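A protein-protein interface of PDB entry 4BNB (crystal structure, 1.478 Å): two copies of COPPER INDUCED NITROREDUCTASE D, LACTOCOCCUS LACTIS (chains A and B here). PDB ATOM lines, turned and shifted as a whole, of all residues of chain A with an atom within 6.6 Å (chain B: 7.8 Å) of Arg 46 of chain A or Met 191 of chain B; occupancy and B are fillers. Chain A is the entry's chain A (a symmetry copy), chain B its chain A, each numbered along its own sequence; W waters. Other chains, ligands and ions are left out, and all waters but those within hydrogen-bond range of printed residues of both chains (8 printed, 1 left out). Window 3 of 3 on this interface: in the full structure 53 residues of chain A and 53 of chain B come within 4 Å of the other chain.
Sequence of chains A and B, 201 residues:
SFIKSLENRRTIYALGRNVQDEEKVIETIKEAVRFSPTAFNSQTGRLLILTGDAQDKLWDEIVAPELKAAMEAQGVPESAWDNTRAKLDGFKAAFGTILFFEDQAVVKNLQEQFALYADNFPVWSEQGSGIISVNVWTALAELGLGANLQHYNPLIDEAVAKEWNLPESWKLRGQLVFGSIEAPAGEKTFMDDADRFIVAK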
ATOM      1  N   VAL A  33      20.510  -8.265  22.000  1.00  0.00           N
ATOM      2  CA  VAL A  33      19.337  -7.481  22.363  1.00  0.00           C
ATOM      3  C   VAL A  33      18.092  -8.007  21.657  1.00  0.00           C
ATOM      4  O   VAL A  33      17.037  -8.164  22.272  1.00  0.00           O
ATOM      5  CB  VAL A  33      19.528  -5.997  22.012  1.00  0.00           C
ATOM      6  CG1 VAL A  33      18.254  -5.215  22.302  1.00  0.00           C
ATOM      7  CG2 VAL A  33      20.713  -5.423  22.784  1.00  0.00           C
ATOM      8  N   ARG A  34      18.226  -8.279  20.364  1.00  0.00           N
ATOM      9  CA  ARG A  34      17.112  -8.749  19.543  1.00  0.00           C
ATOM     10  C   ARG A  34      16.434  -9.972  20.152  1.00  0.00           C
ATOM     11  O   ARG A  34      15.209 -10.056  20.217  1.00  0.00           O
ATOM     12  CB  ARG A  34      17.621  -9.099  18.143  1.00  0.00           C
ATOM     13  CG  ARG A  34      16.547  -9.581  17.183  1.00  0.00           C
ATOM     14  CD  ARG A  34      17.145  -9.996  15.849  1.00  0.00           C
ATOM     15  NE  ARG A  34      16.121 -10.139  14.818  1.00  0.00           N
ATOM     16  CZ  ARG A  34      15.639  -9.137  14.090  1.00  0.00           C
ATOM     17  NH1 ARG A  34      16.079  -7.899  14.266  1.00  0.00           N
ATOM     18  NH2 ARG A  34      14.706  -9.374  13.185  1.00  0.00           N
ATOM     19  N   ASN A  41       6.443  -8.230  24.648  1.00  0.00           N
ATOM     20  CA  ASN A  41       7.330  -8.037  23.506  1.00  0.00           C
ATOM     21  C   ASN A  41       7.490  -6.553  23.205  1.00  0.00           C
ATOM     22  O   ASN A  41       7.575  -6.147  22.042  1.00  0.00           O
ATOM     23  CB  ASN A  41       6.798  -8.764  22.267  1.00  0.00           C
ATOM     24  CG  ASN A  41       7.850  -8.907  21.180  1.00  0.00           C
ATOM     25  OD1 ASN A  41       9.042  -9.033  21.466  1.00  0.00           O
ATOM     26  ND2 ASN A  41       7.414  -8.891  19.926  1.00  0.00           N
ATOM     27  N   SER A  42       7.547  -5.748  24.261  1.00  0.00           N
ATOM     28  CA  SER A  42       7.570  -4.294  24.136  1.00  0.00           C
ATOM     29  C   SER A  42       8.924  -3.749  23.666  1.00  0.00           C
ATOM     30  O   SER A  42       9.003  -2.632  23.158  1.00  0.00           O
ATOM     31  CB  SER A  42       7.179  -3.650  25.470  1.00  0.00           C
ATOM     32  OG  SER A  42       8.030  -4.086  26.516  1.00  0.00           O
ATOM     33  N   GLN A  43       9.987  -4.525  23.856  1.00  0.00           N
ATOM     34  CA  GLN A  43      11.295  -4.171  23.311  1.00  0.00           C
ATOM     35  C   GLN A  43      11.658  -2.731  23.628  1.00  0.00           C
ATOM     36  O   GLN A  43      11.977  -1.947  22.734  1.00  0.00           O
ATOM     37  CB  GLN A  43      11.290  -4.372  21.798  1.00  0.00           C
ATOM     38  CG  GLN A  43      11.042  -5.807  21.381  1.00  0.00           C
ATOM     39  CD  GLN A  43      10.702  -5.920  19.913  1.00  0.00           C
ATOM     40  OE1 GLN A  43      11.572  -5.794  19.055  1.00  0.00           O
ATOM     41  NE2 GLN A  43       9.426  -6.146  19.617  1.00  0.00           N
ATOM     42  N   THR A  44      11.631  -2.395  24.912  1.00  0.00           N
ATOM     43  CA  THR A  44      11.808  -1.019  25.356  1.00  0.00           C
ATOM     44  C   THR A  44      13.270  -0.581  25.408  1.00  0.00           C
ATOM     45  O   THR A  44      13.560   0.600  25.606  1.00  0.00           O
ATOM     46  CB  THR A  44      11.190  -0.842  26.746  1.00  0.00           C
ATOM     47  OG1 THR A  44      11.550  -1.962  27.565  1.00  0.00           O
ATOM     48  CG2 THR A  44       9.677  -0.768  26.643  1.00  0.00           C
ATOM     49  N   GLY A  45      14.189  -1.523  25.228  1.00  0.00           N
ATOM     50  CA  GLY A  45      15.607  -1.216  25.276  1.00  0.00           C
ATOM     51  C   GLY A  45      16.083  -0.405  24.083  1.00  0.00           C
ATOM     52  O   GLY A  45      15.663  -0.640  22.945  1.00  0.00           O
ATOM     53  N   ARG A  46      16.964   0.555  24.352  1.00  0.00           N
ATOM     54  CA  ARG A  46      17.589   1.362  23.311  1.00  0.00           C
ATOM     55  C   ARG A  46      19.083   1.415  23.595  1.00  0.00           C
ATOM     56  O   ARG A  46      19.487   1.506  24.753  1.00  0.00           O
ATOM     57  CB  ARG A  46      17.021   2.781  23.307  1.00  0.00           C
ATOM     58  CG  ARG A  46      15.504   2.866  23.197  1.00  0.00           C
ATOM     59  CD  ARG A  46      15.017   2.597  21.778  1.00  0.00           C
ATOM     60  NE  ARG A  46      13.558   2.660  21.692  1.00  0.00           N
ATOM     61  CZ  ARG A  46      12.744   1.613  21.813  1.00  0.00           C
ATOM     62  NH1 ARG A  46      13.224   0.392  22.016  1.00  0.00           N
ATOM     63  NH2 ARG A  46      11.432   1.789  21.726  1.00  0.00           N
ATOM     64  N   LEU A  47      19.900   1.356  22.548  1.00  0.00           N
ATOM     65  CA  LEU A  47      21.350   1.368  22.708  1.00  0.00           C
ATOM     66  C   LEU A  47      22.013   2.484  21.920  1.00  0.00           C
ATOM     67  O   LEU A  47      21.679   2.721  20.757  1.00  0.00           O
ATOM     68  CB  LEU A  47      21.955   0.039  22.253  1.00  0.00           C
ATOM     69  CG  LEU A  47      21.948  -1.131  23.235  1.00  0.00           C
ATOM     70  CD1 LEU A  47      20.531  -1.591  23.531  1.00  0.00           C
ATOM     71  CD2 LEU A  47      22.776  -2.268  22.660  1.00  0.00           C
ATOM     72  N   LEU A  48      22.952   3.164  22.571  1.00  0.00           N
ATOM     73  CA  LEU A  48      23.917   4.014  21.894  1.00  0.00           C
ATOM     74  C   LEU A  48      25.283   3.349  22.044  1.00  0.00           C
ATOM     75  O   LEU A  48      25.776   3.164  23.156  1.00  0.00           O
ATOM     76  CB  LEU A  48      23.927   5.421  22.495  1.00  0.00           C
ATOM     77  CG  LEU A  48      24.986   6.383  21.958  1.00  0.00           C
ATOM     78  CD1 LEU A  48      24.756   6.677  20.481  1.00  0.00           C
ATOM     79  CD2 LEU A  48      24.987   7.668  22.771  1.00  0.00           C
ATOM     80  N   LEU A  99      25.774   2.322  25.823  1.00  0.00           N
ATOM     81  CA  LEU A  99      24.863   2.963  26.758  1.00  0.00           C
ATOM     82  C   LEU A  99      23.462   2.389  26.576  1.00  0.00           C
ATOM     83  O   LEU A  99      22.908   2.403  25.476  1.00  0.00           O
ATOM     84  CB  LEU A  99      24.875   4.487  26.582  1.00  0.00           C
ATOM     85  CG  LEU A  99      26.213   5.169  26.901  1.00  0.00           C
ATOM     86  CD1 LEU A  99      27.146   5.160  25.693  1.00  0.00           C
ATOM     87  CD2 LEU A  99      26.002   6.592  27.405  1.00  0.00           C
ATOM     88  N   PHE A 100      22.915   1.860  27.664  1.00  0.00           N
ATOM     89  CA  PHE A 100      21.611   1.209  27.653  1.00  0.00           C
ATOM     90  C   PHE A 100      20.548   2.152  28.197  1.00  0.00           C
ATOM     91  O   PHE A 100      20.686   2.677  29.301  1.00  0.00           O
ATOM     92  CB  PHE A 100      21.642  -0.061  28.511  1.00  0.00           C
ATOM     93  CG  PHE A 100      22.411  -1.197  27.892  1.00  0.00           C
ATOM     94  CD1 PHE A 100      23.770  -1.342  28.118  1.00  0.00           C
ATOM     95  CD2 PHE A 100      21.770  -2.124  27.088  1.00  0.00           C
ATOM     96  CE1 PHE A 100      24.473  -2.390  27.553  1.00  0.00           C
ATOM     97  CE2 PHE A 100      22.471  -3.174  26.520  1.00  0.00           C
ATOM     98  CZ  PHE A 100      23.822  -3.308  26.754  1.00  0.00           C
ATOM     99  N   PHE A 101      19.491   2.356  27.416  1.00  0.00           N
ATOM    100  CA  PHE A 101      18.362   3.180  27.825  1.00  0.00           C
ATOM    101  C   PHE A 101      17.076   2.368  27.791  1.00  0.00           C
ATOM    102  O   PHE A 101      17.000   1.321  27.138  1.00  0.00           O
ATOM    103  CB  PHE A 101      18.163   4.373  26.882  1.00  0.00           C
ATOM    104  CG  PHE A 101      19.400   5.184  26.624  1.00  0.00           C
ATOM    105  CD1 PHE A 101      20.405   4.700  25.800  1.00  0.00           C
ATOM    106  CD2 PHE A 101      19.535   6.453  27.167  1.00  0.00           C
ATOM    107  CE1 PHE A 101      21.535   5.455  25.544  1.00  0.00           C
ATOM    108  CE2 PHE A 101      20.660   7.219  26.911  1.00  0.00           C
ATOM    109  CZ  PHE A 101      21.664   6.717  26.101  1.00  0.00           C
ATOM    110  N   GLU A 102      16.057   2.875  28.477  1.00  0.00           N
ATOM    111  CA  GLU A 102      14.707   2.335  28.367  1.00  0.00           C
ATOM    112  C   GLU A 102      13.784   3.430  27.849  1.00  0.00           C
ATOM    113  O   GLU A 102      13.775   4.543  28.374  1.00  0.00           O
ATOM    114  CB  GLU A 102      14.223   1.812  29.722  1.00  0.00           C
ATOM    115  CG  GLU A 102      14.872   0.495  30.138  1.00  0.00           C
ATOM    116  CD  GLU A 102      14.421  -0.670  29.274  1.00  0.00           C
ATOM    117  OE1 GLU A 102      13.193  -0.848  29.119  1.00  0.00           O
ATOM    118  OE2 GLU A 102      15.289  -1.397  28.741  1.00  0.00           O
ATOM    119  N   ASP A 103      13.021   3.113  26.808  1.00  0.00           N
ATOM    120  CA  ASP A 103      12.169   4.099  26.150  1.00  0.00           C
ATOM    121  C   ASP A 103      10.898   4.356  26.961  1.00  0.00           C
ATOM    122  O   ASP A 103       9.970   3.548  26.965  1.00  0.00           O
ATOM    123  CB  ASP A 103      11.814   3.627  24.738  1.00  0.00           C
ATOM    124  CG  ASP A 103      11.159   4.711  23.911  1.00  0.00           C
ATOM    125  OD1 ASP A 103      10.514   5.600  24.502  1.00  0.00           O
ATOM    126  OD2 ASP A 103      11.289   4.676  22.668  1.00  0.00           O
ATOM    127  N   VAL A 106       7.307   4.350  25.282  1.00  0.00           N
ATOM    128  CA  VAL A 106       6.673   3.046  25.135  1.00  0.00           C
ATOM    129  C   VAL A 106       6.102   2.591  26.475  1.00  0.00           C
ATOM    130  O   VAL A 106       4.995   2.065  26.537  1.00  0.00           O
ATOM    131  CB  VAL A 106       7.662   1.995  24.603  1.00  0.00           C
ATOM    132  CG1 VAL A 106       7.023   0.612  24.593  1.00  0.00           C
ATOM    133  CG2 VAL A 106       8.134   2.373  23.208  1.00  0.00           C
ATOM    134  N   ILE A 132      18.899  -7.273  28.866  1.00  0.00           N
ATOM    135  CA  ILE A 132      19.662  -7.021  27.648  1.00  0.00           C
ATOM    136  C   ILE A 132      21.108  -6.652  27.974  1.00  0.00           C
ATOM    137  O   ILE A 132      22.016  -6.967  27.214  1.00  0.00           O
ATOM    138  CB  ILE A 132      18.995  -5.972  26.724  1.00  0.00           C
ATOM    139  CG1 ILE A 132      18.897  -4.603  27.399  1.00  0.00           C
ATOM    140  CG2 ILE A 132      17.613  -6.458  26.289  1.00  0.00           C
ATOM    141  CD1 ILE A 132      18.464  -3.501  26.441  1.00  0.00           C
ATOM    142  N   SER A 169      12.804  10.688  25.411  1.00  0.00           N
ATOM    143  CA  SER A 169      12.155   9.538  26.035  1.00  0.00           C
ATOM    144  C   SER A 169      13.131   8.418  26.402  1.00  0.00           C
ATOM    145  O   SER A 169      12.763   7.501  27.132  1.00  0.00           O
ATOM    146  CB  SER A 169      11.046   8.989  25.131  1.00  0.00           C
ATOM    147  OG  SER A 169      11.574   8.401  23.956  1.00  0.00           O
ATOM    148  N   TRP A 170      14.364   8.479  25.902  1.00  0.00           N
ATOM    149  CA  TRP A 170      15.366   7.475  26.264  1.00  0.00           C
ATOM    150  C   TRP A 170      15.915   7.738  27.664  1.00  0.00           C
ATOM    151  O   TRP A 170      16.585   8.745  27.900  1.00  0.00           O
ATOM    152  CB  TRP A 170      16.532   7.459  25.273  1.00  0.00           C
ATOM    153  CG  TRP A 170      16.207   6.911  23.913  1.00  0.00           C
ATOM    154  CD1 TRP A 170      14.978   6.835  23.321  1.00  0.00           C
ATOM    155  CD2 TRP A 170      17.138   6.368  22.972  1.00  0.00           C
ATOM    156  NE1 TRP A 170      15.090   6.281  22.067  1.00  0.00           N
ATOM    157  CE2 TRP A 170      16.406   5.983  21.832  1.00  0.00           C
ATOM    158  CE3 TRP A 170      18.523   6.169  22.984  1.00  0.00           C
ATOM    159  CZ2 TRP A 170      17.012   5.413  20.713  1.00  0.00           C
ATOM    160  CZ3 TRP A 170      19.121   5.603  21.874  1.00  0.00           C
ATOM    161  CH2 TRP A 170      18.368   5.231  20.755  1.00  0.00           C
ATOM    162  N   THR B 189       7.418 -10.847  16.355  1.00  0.00           N
ATOM    163  CA  THR B 189       7.971  -9.787  15.522  1.00  0.00           C
ATOM    164  C   THR B 189       9.104  -9.062  16.240  1.00  0.00           C
ATOM    165  O   THR B 189       9.281  -9.206  17.453  1.00  0.00           O
ATOM    166  CB  THR B 189       6.896  -8.756  15.127  1.00  0.00           C
ATOM    167  OG1 THR B 189       6.335  -8.168  16.306  1.00  0.00           O
ATOM    168  CG2 THR B 189       5.789  -9.420  14.319  1.00  0.00           C
ATOM    169  N   PHE B 190       9.869  -8.288  15.477  1.00  0.00           N
ATOM    170  CA  PHE B 190      10.976  -7.506  16.013  1.00  0.00           C
ATOM    171  C   PHE B 190      10.895  -6.077  15.491  1.00  0.00           C
ATOM    172  O   PHE B 190      10.461  -5.848  14.358  1.00  0.00           O
ATOM    173  CB  PHE B 190      12.318  -8.116  15.589  1.00  0.00           C
ATOM    174  CG  PHE B 190      12.495  -9.553  15.997  1.00  0.00           C
ATOM    175  CD1 PHE B 190      12.047 -10.579  15.182  1.00  0.00           C
ATOM    176  CD2 PHE B 190      13.121  -9.877  17.188  1.00  0.00           C
ATOM    177  CE1 PHE B 190      12.210 -11.903  15.552  1.00  0.00           C
ATOM    178  CE2 PHE B 190      13.290 -11.198  17.562  1.00  0.00           C
ATOM    179  CZ  PHE B 190      12.835 -12.210  16.746  1.00  0.00           C
ATOM    180  N   MET B 191      11.305  -5.123  16.324  1.00  0.00           N
ATOM    181  CA  MET B 191      11.473  -3.733  15.909  1.00  0.00           C
ATOM    182  C   MET B 191      12.446  -3.580  14.753  1.00  0.00           C
ATOM    183  O   MET B 191      13.272  -4.450  14.496  1.00  0.00           O
ATOM    184  CB  MET B 191      12.077  -2.917  17.046  1.00  0.00           C
ATOM    185  CG  MET B 191      11.156  -2.518  18.154  1.00  0.00           C
ATOM    186  SD  MET B 191      12.108  -1.496  19.286  1.00  0.00           S
ATOM    187  CE  MET B 191      12.347  -0.021  18.304  1.00  0.00           C
ATOM    188  N   ASP B 192      12.358  -2.432  14.093  1.00  0.00           N
ATOM    189  CA  ASP B 192      13.368  -1.985  13.144  1.00  0.00           C
ATOM    190  C   ASP B 192      14.644  -1.652  13.922  1.00  0.00           C
ATOM    191  O   ASP B 192      14.601  -0.889  14.886  1.00  0.00           O
ATOM    192  CB  ASP B 192      12.836  -0.743  12.418  1.00  0.00           C
ATOM    193  CG  ASP B 192      13.733  -0.273  11.289  1.00  0.00           C
ATOM    194  OD1 ASP B 192      14.925  -0.634  11.246  1.00  0.00           O
ATOM    195  OD2 ASP B 192      13.227   0.484  10.433  1.00  0.00           O
ATOM    196  N   ASP B 193      15.772  -2.238  13.522  1.00  0.00           N
ATOM    197  CA  ASP B 193      17.067  -1.913  14.127  1.00  0.00           C
ATOM    198  C   ASP B 193      17.268  -0.403  14.248  1.00  0.00           C
ATOM    199  O   ASP B 193      17.822   0.079  15.234  1.00  0.00           O
ATOM    200  CB  ASP B 193      18.228  -2.467  13.291  1.00  0.00           C
ATOM    201  CG  ASP B 193      18.434  -3.959  13.460  1.00  0.00           C
ATOM    202  OD1 ASP B 193      17.818  -4.568  14.359  1.00  0.00           O
ATOM    203  OD2 ASP B 193      19.236  -4.523  12.680  1.00  0.00           O
ATOM    204  N   ALA B 194      16.841   0.337  13.229  1.00  0.00           N
ATOM    205  CA  ALA B 194      17.127   1.763  13.153  1.00  0.00           C
ATOM    206  C   ALA B 194      16.465   2.542  14.281  1.00  0.00           C
ATOM    207  O   ALA B 194      16.893   3.648  14.611  1.00  0.00           O
ATOM    208  CB  ALA B 194      16.692   2.315  11.800  1.00  0.00           C
ATOM    209  N   ASP B 195      15.429   1.962  14.880  1.00  0.00           N
ATOM    210  CA  ASP B 195      14.689   2.640  15.939  1.00  0.00           C
ATOM    211  C   ASP B 195      15.222   2.351  17.348  1.00  0.00           C
ATOM    212  O   ASP B 195      14.798   2.999  18.308  1.00  0.00           O
ATOM    213  CB  ASP B 195      13.202   2.284  15.863  1.00  0.00           C
ATOM    214  CG  ASP B 195      12.530   2.839  14.619  1.00  0.00           C
ATOM    215  OD1 ASP B 195      12.955   3.909  14.130  1.00  0.00           O
ATOM    216  OD2 ASP B 195      11.571   2.205  14.131  1.00  0.00           O
ATOM    217  N   ARG B 196      16.137   1.393  17.492  1.00  0.00           N
ATOM    218  CA  ARG B 196      16.672   1.090  18.823  1.00  0.00           C
ATOM    219  C   ARG B 196      18.196   0.974  18.932  1.00  0.00           C
ATOM    220  O   ARG B 196      18.714   0.855  20.040  1.00  0.00           O
ATOM    221  CB  ARG B 196      16.013  -0.164  19.411  1.00  0.00           C
ATOM    222  CG  ARG B 196      16.225  -1.443  18.621  1.00  0.00           C
ATOM    223  CD  ARG B 196      15.807  -2.648  19.456  1.00  0.00           C
ATOM    224  NE  ARG B 196      15.581  -3.831  18.640  1.00  0.00           N
ATOM    225  CZ  ARG B 196      15.091  -4.978  19.098  1.00  0.00           C
ATOM    226  NH1 ARG B 196      14.782  -5.111  20.381  1.00  0.00           N
ATOM    227  NH2 ARG B 196      14.911  -5.999  18.271  1.00  0.00           N
ATOM    228  N   PHE B 197      18.909   1.012  17.809  1.00  0.00           N
ATOM    229  CA  PHE B 197      20.371   1.000  17.842  1.00  0.00           C
ATOM    230  C   PHE B 197      20.954   2.204  17.114  1.00  0.00           C
ATOM    231  O   PHE B 197      20.650   2.447  15.948  1.00  0.00           O
ATOM    232  CB  PHE B 197      20.951  -0.271  17.204  1.00  0.00           C
ATOM    233  CG  PHE B 197      20.373  -1.552  17.736  1.00  0.00           C
ATOM    234  CD1 PHE B 197      20.621  -1.957  19.034  1.00  0.00           C
ATOM    235  CD2 PHE B 197      19.607  -2.365  16.921  1.00  0.00           C
ATOM    236  CE1 PHE B 197      20.097  -3.141  19.515  1.00  0.00           C
ATOM    237  CE2 PHE B 197      19.080  -3.548  17.396  1.00  0.00           C
ATOM    238  CZ  PHE B 197      19.326  -3.938  18.693  1.00  0.00           C
ATOM    239  N   ILE B 198      21.798   2.951  17.818  1.00  0.00           N
ATOM    240  CA  ILE B 198      22.578   4.018  17.213  1.00  0.00           C
ATOM    241  C   ILE B 198      24.053   3.705  17.422  1.00  0.00           C
ATOM    242  O   ILE B 198      24.488   3.451  18.546  1.00  0.00           O
ATOM    243  CB  ILE B 198      22.273   5.384  17.843  1.00  0.00           C
ATOM    244  CG1 ILE B 198      20.802   5.750  17.638  1.00  0.00           C
ATOM    245  CG2 ILE B 198      23.174   6.456  17.242  1.00  0.00           C
ATOM    246  CD1 ILE B 198      20.367   6.977  18.411  1.00  0.00           C
HETATM  247  O   HOH W   1      13.678  -7.870  20.049  1.00  0.00           O
HETATM  248  O   HOH W   2      18.626  -6.863  15.560  1.00  0.00           O
HETATM  249  O   HOH W   3      11.118  -9.182  19.718  1.00  0.00           O
HETATM  250  O   HOH W   4       5.012 -10.346  18.151  1.00  0.00           O
HETATM  251  O   HOH W   5       4.563  -8.221  19.317  1.00  0.00           O
HETATM  252  O   HOH W   6       7.736  -5.858  17.076  1.00  0.00           O
HETATM  253  O   HOH W   7      15.275  -3.402  22.547  1.00  0.00           O
HETATM  254  O   HOH W   8      13.317   5.189  19.914  1.00  0.00           O
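The side-chain amide nitrogen of Asn 41 of chain A sits at hydrogen-bond distance from the backbone carbonyl oxygen of Thr 189 of chain B (3.1 Å).
N of Met 191 of chain B is in hydrogen-bond range of OE1 of Gln 43 of chain A (2.8 Å).
The side-chain sulfur (SD) of Met 191 of chain B sits at hydrogen-bond distance from the guanidinium group (NH1) of Arg 46 of chain A, 3.5 Å away.
OD1 of Asp 193 of chain B lies within salt-bridge range of NH1 of Arg 34 of chain A, at 3.8 Å.
The guanidinium group (NH2) of Arg 196 of chain B is in hydrogen-bond range of the side-chain amide oxygen (OE1) of Gln 43 of chain A, at 3.4 Å.
O of Arg 196 of chain B sits at hydrogen-bond distance from N of Leu 47 of chain A.
N of Ile 198 of chain B lies within hydrogen-bond range of O of Leu 47 of chain A (3.0 Å).
Of the printed residues of chain B, Arg 34 of chain A touches Phe 190 (3.4 Å), Asp 193 (3.8 Å) and Arg 196 (3.7 Å).
Of the printed residues of chain B, Gln 43 of chain A touches Thr 189 (3.8 Å), Phe 190 (3.5 Å), Met 191 (2.8 Å) and Arg 196 (3.4 Å).
Gly 45 of chain A touches just one residue of chain B: Arg 196 (3.6 Å).
Of chain B, only Met 191 (3.5 Å), Asp 195 (3.5 Å) and Arg 196 (3.5 Å) come within 4 Å of Arg 46 of chain A.
Of the printed residues of chain B, Leu 48 of chain A touches Ile 198.
Printed residues of chain A within 4 Å of Met 191 of chain B: Gln 43 (2.8 Å) and Arg 46 (3.5 Å).
Of the printed residues of chain A, Phe 197 of chain B touches Val 33 (3.8 Å) and Leu 47 (3.6 Å).
The nearest residue of chain A that does not touch Met 191 of chain B is Arg 34 of chain A (4.5 Å).
Water W1 lies within hydrogen-bond range of the backbone carbonyl oxygen (O) of Arg 34 of chain A, the guanidinium group (NH2) of Arg 196 of chain B and the side-chain amide oxygen (OE1) of Gln 43 of chain A.
Water W2 bridges the side-chain carboxylate of Asp 193 of chain B and the guanidinium group of Arg 34 of chain A.
Water W3 lies within hydrogen-bond range of OD1 of Asn 41 of chain A (2.7 Å), O of Thr 189 of chain B (2.9 Å) and NE2 of Gln 43 of chain A (3.5 Å).
Water W6 bridges OG1 of Thr 189 of chain B and NE2 of Gln 43 of chain A.
Water W8 lies within hydrogen-bond range of NE1 of Trp 170 of chain A (3.0 Å), O of Asp 195 of chain B (3.1 Å), NE of Arg 46 of chain A (3.1 Å) and OD2 of Asp 103 of chain A (3.5 Å).
Water W4 bridges N of Thr 189 of chain B (3.0 Å) and ND2 of Asn 41 of chain A (3.3 Å).
O of Asn 41 of chain A is in hydrogen-bond range of NE2 of Gln 43 of chain A (3.1 Å).
The guanidinium group (NH1) of Arg 46 of chain A sits at hydrogen-bond distance from the backbone carbonyl oxygen (O) of Gln 43 of chain A (2.7 Å).
O of Arg 46 of chain A lies within hydrogen-bond range of N of Phe 101 of chain A, 2.8 Å away.
NH2 of Arg 46 of chain A lies within salt-bridge range of OD2 of Asp 103 of chain A, 3.0 Å away.
O of Leu 48 of chain A lies within hydrogen-bond range of N of Leu 99 of chain A (2.8 Å).
No position is printed for both chains.
Of the 19 pairs that touch across the chains among the printed residues, none has its exchanged pair printed and touching as well.
Of the 10 printed residues of chain B, 8 touch a printed residue of chain A.
Hydrophobic or aromatic side chains of chain B within 4 Å of the printed part of chain A: Phe 190, Met 191, Phe 197 and Ile 198.
Among the printed residues, Asp or Glu carboxylates within 4 Å of a Lys or Arg side-chain nitrogen of the other chain: Arg 34 of chain A with Asp 193 of chain B (3.8 Å).
Among the printed residues, merely in contact across the chains: Val 33 of chain A with Arg 196 of chain B (3.97 Å), Val 33 of chain A with Phe 197 of chain B (3.8 Å), Arg 34 of chain A with Phe 190 of chain B (3.4 Å), Arg 34 of chain A with Arg 196 of chain B (3.7 Å), Gln 43 of chain A with Thr 189 of chain B (3.8 Å), Gln 43 of chain A with Phe 190 of chain B (3.5 Å), Gly 45 of chain A with Arg 196 of chain B (3.6 Å), Arg 46 of chain A with Asp 195 of chain B (3.5 Å), Arg 46 of chain A with Arg 196 of chain B (3.5 Å), Leu 47 of chain A with Phe 197 of chain B (3.6 Å), Leu 48 of chain A with Ile 198 of chain B (3.4 Å) and Trp 170 of chain A with Ile 198 of chain B (3.5 Å).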
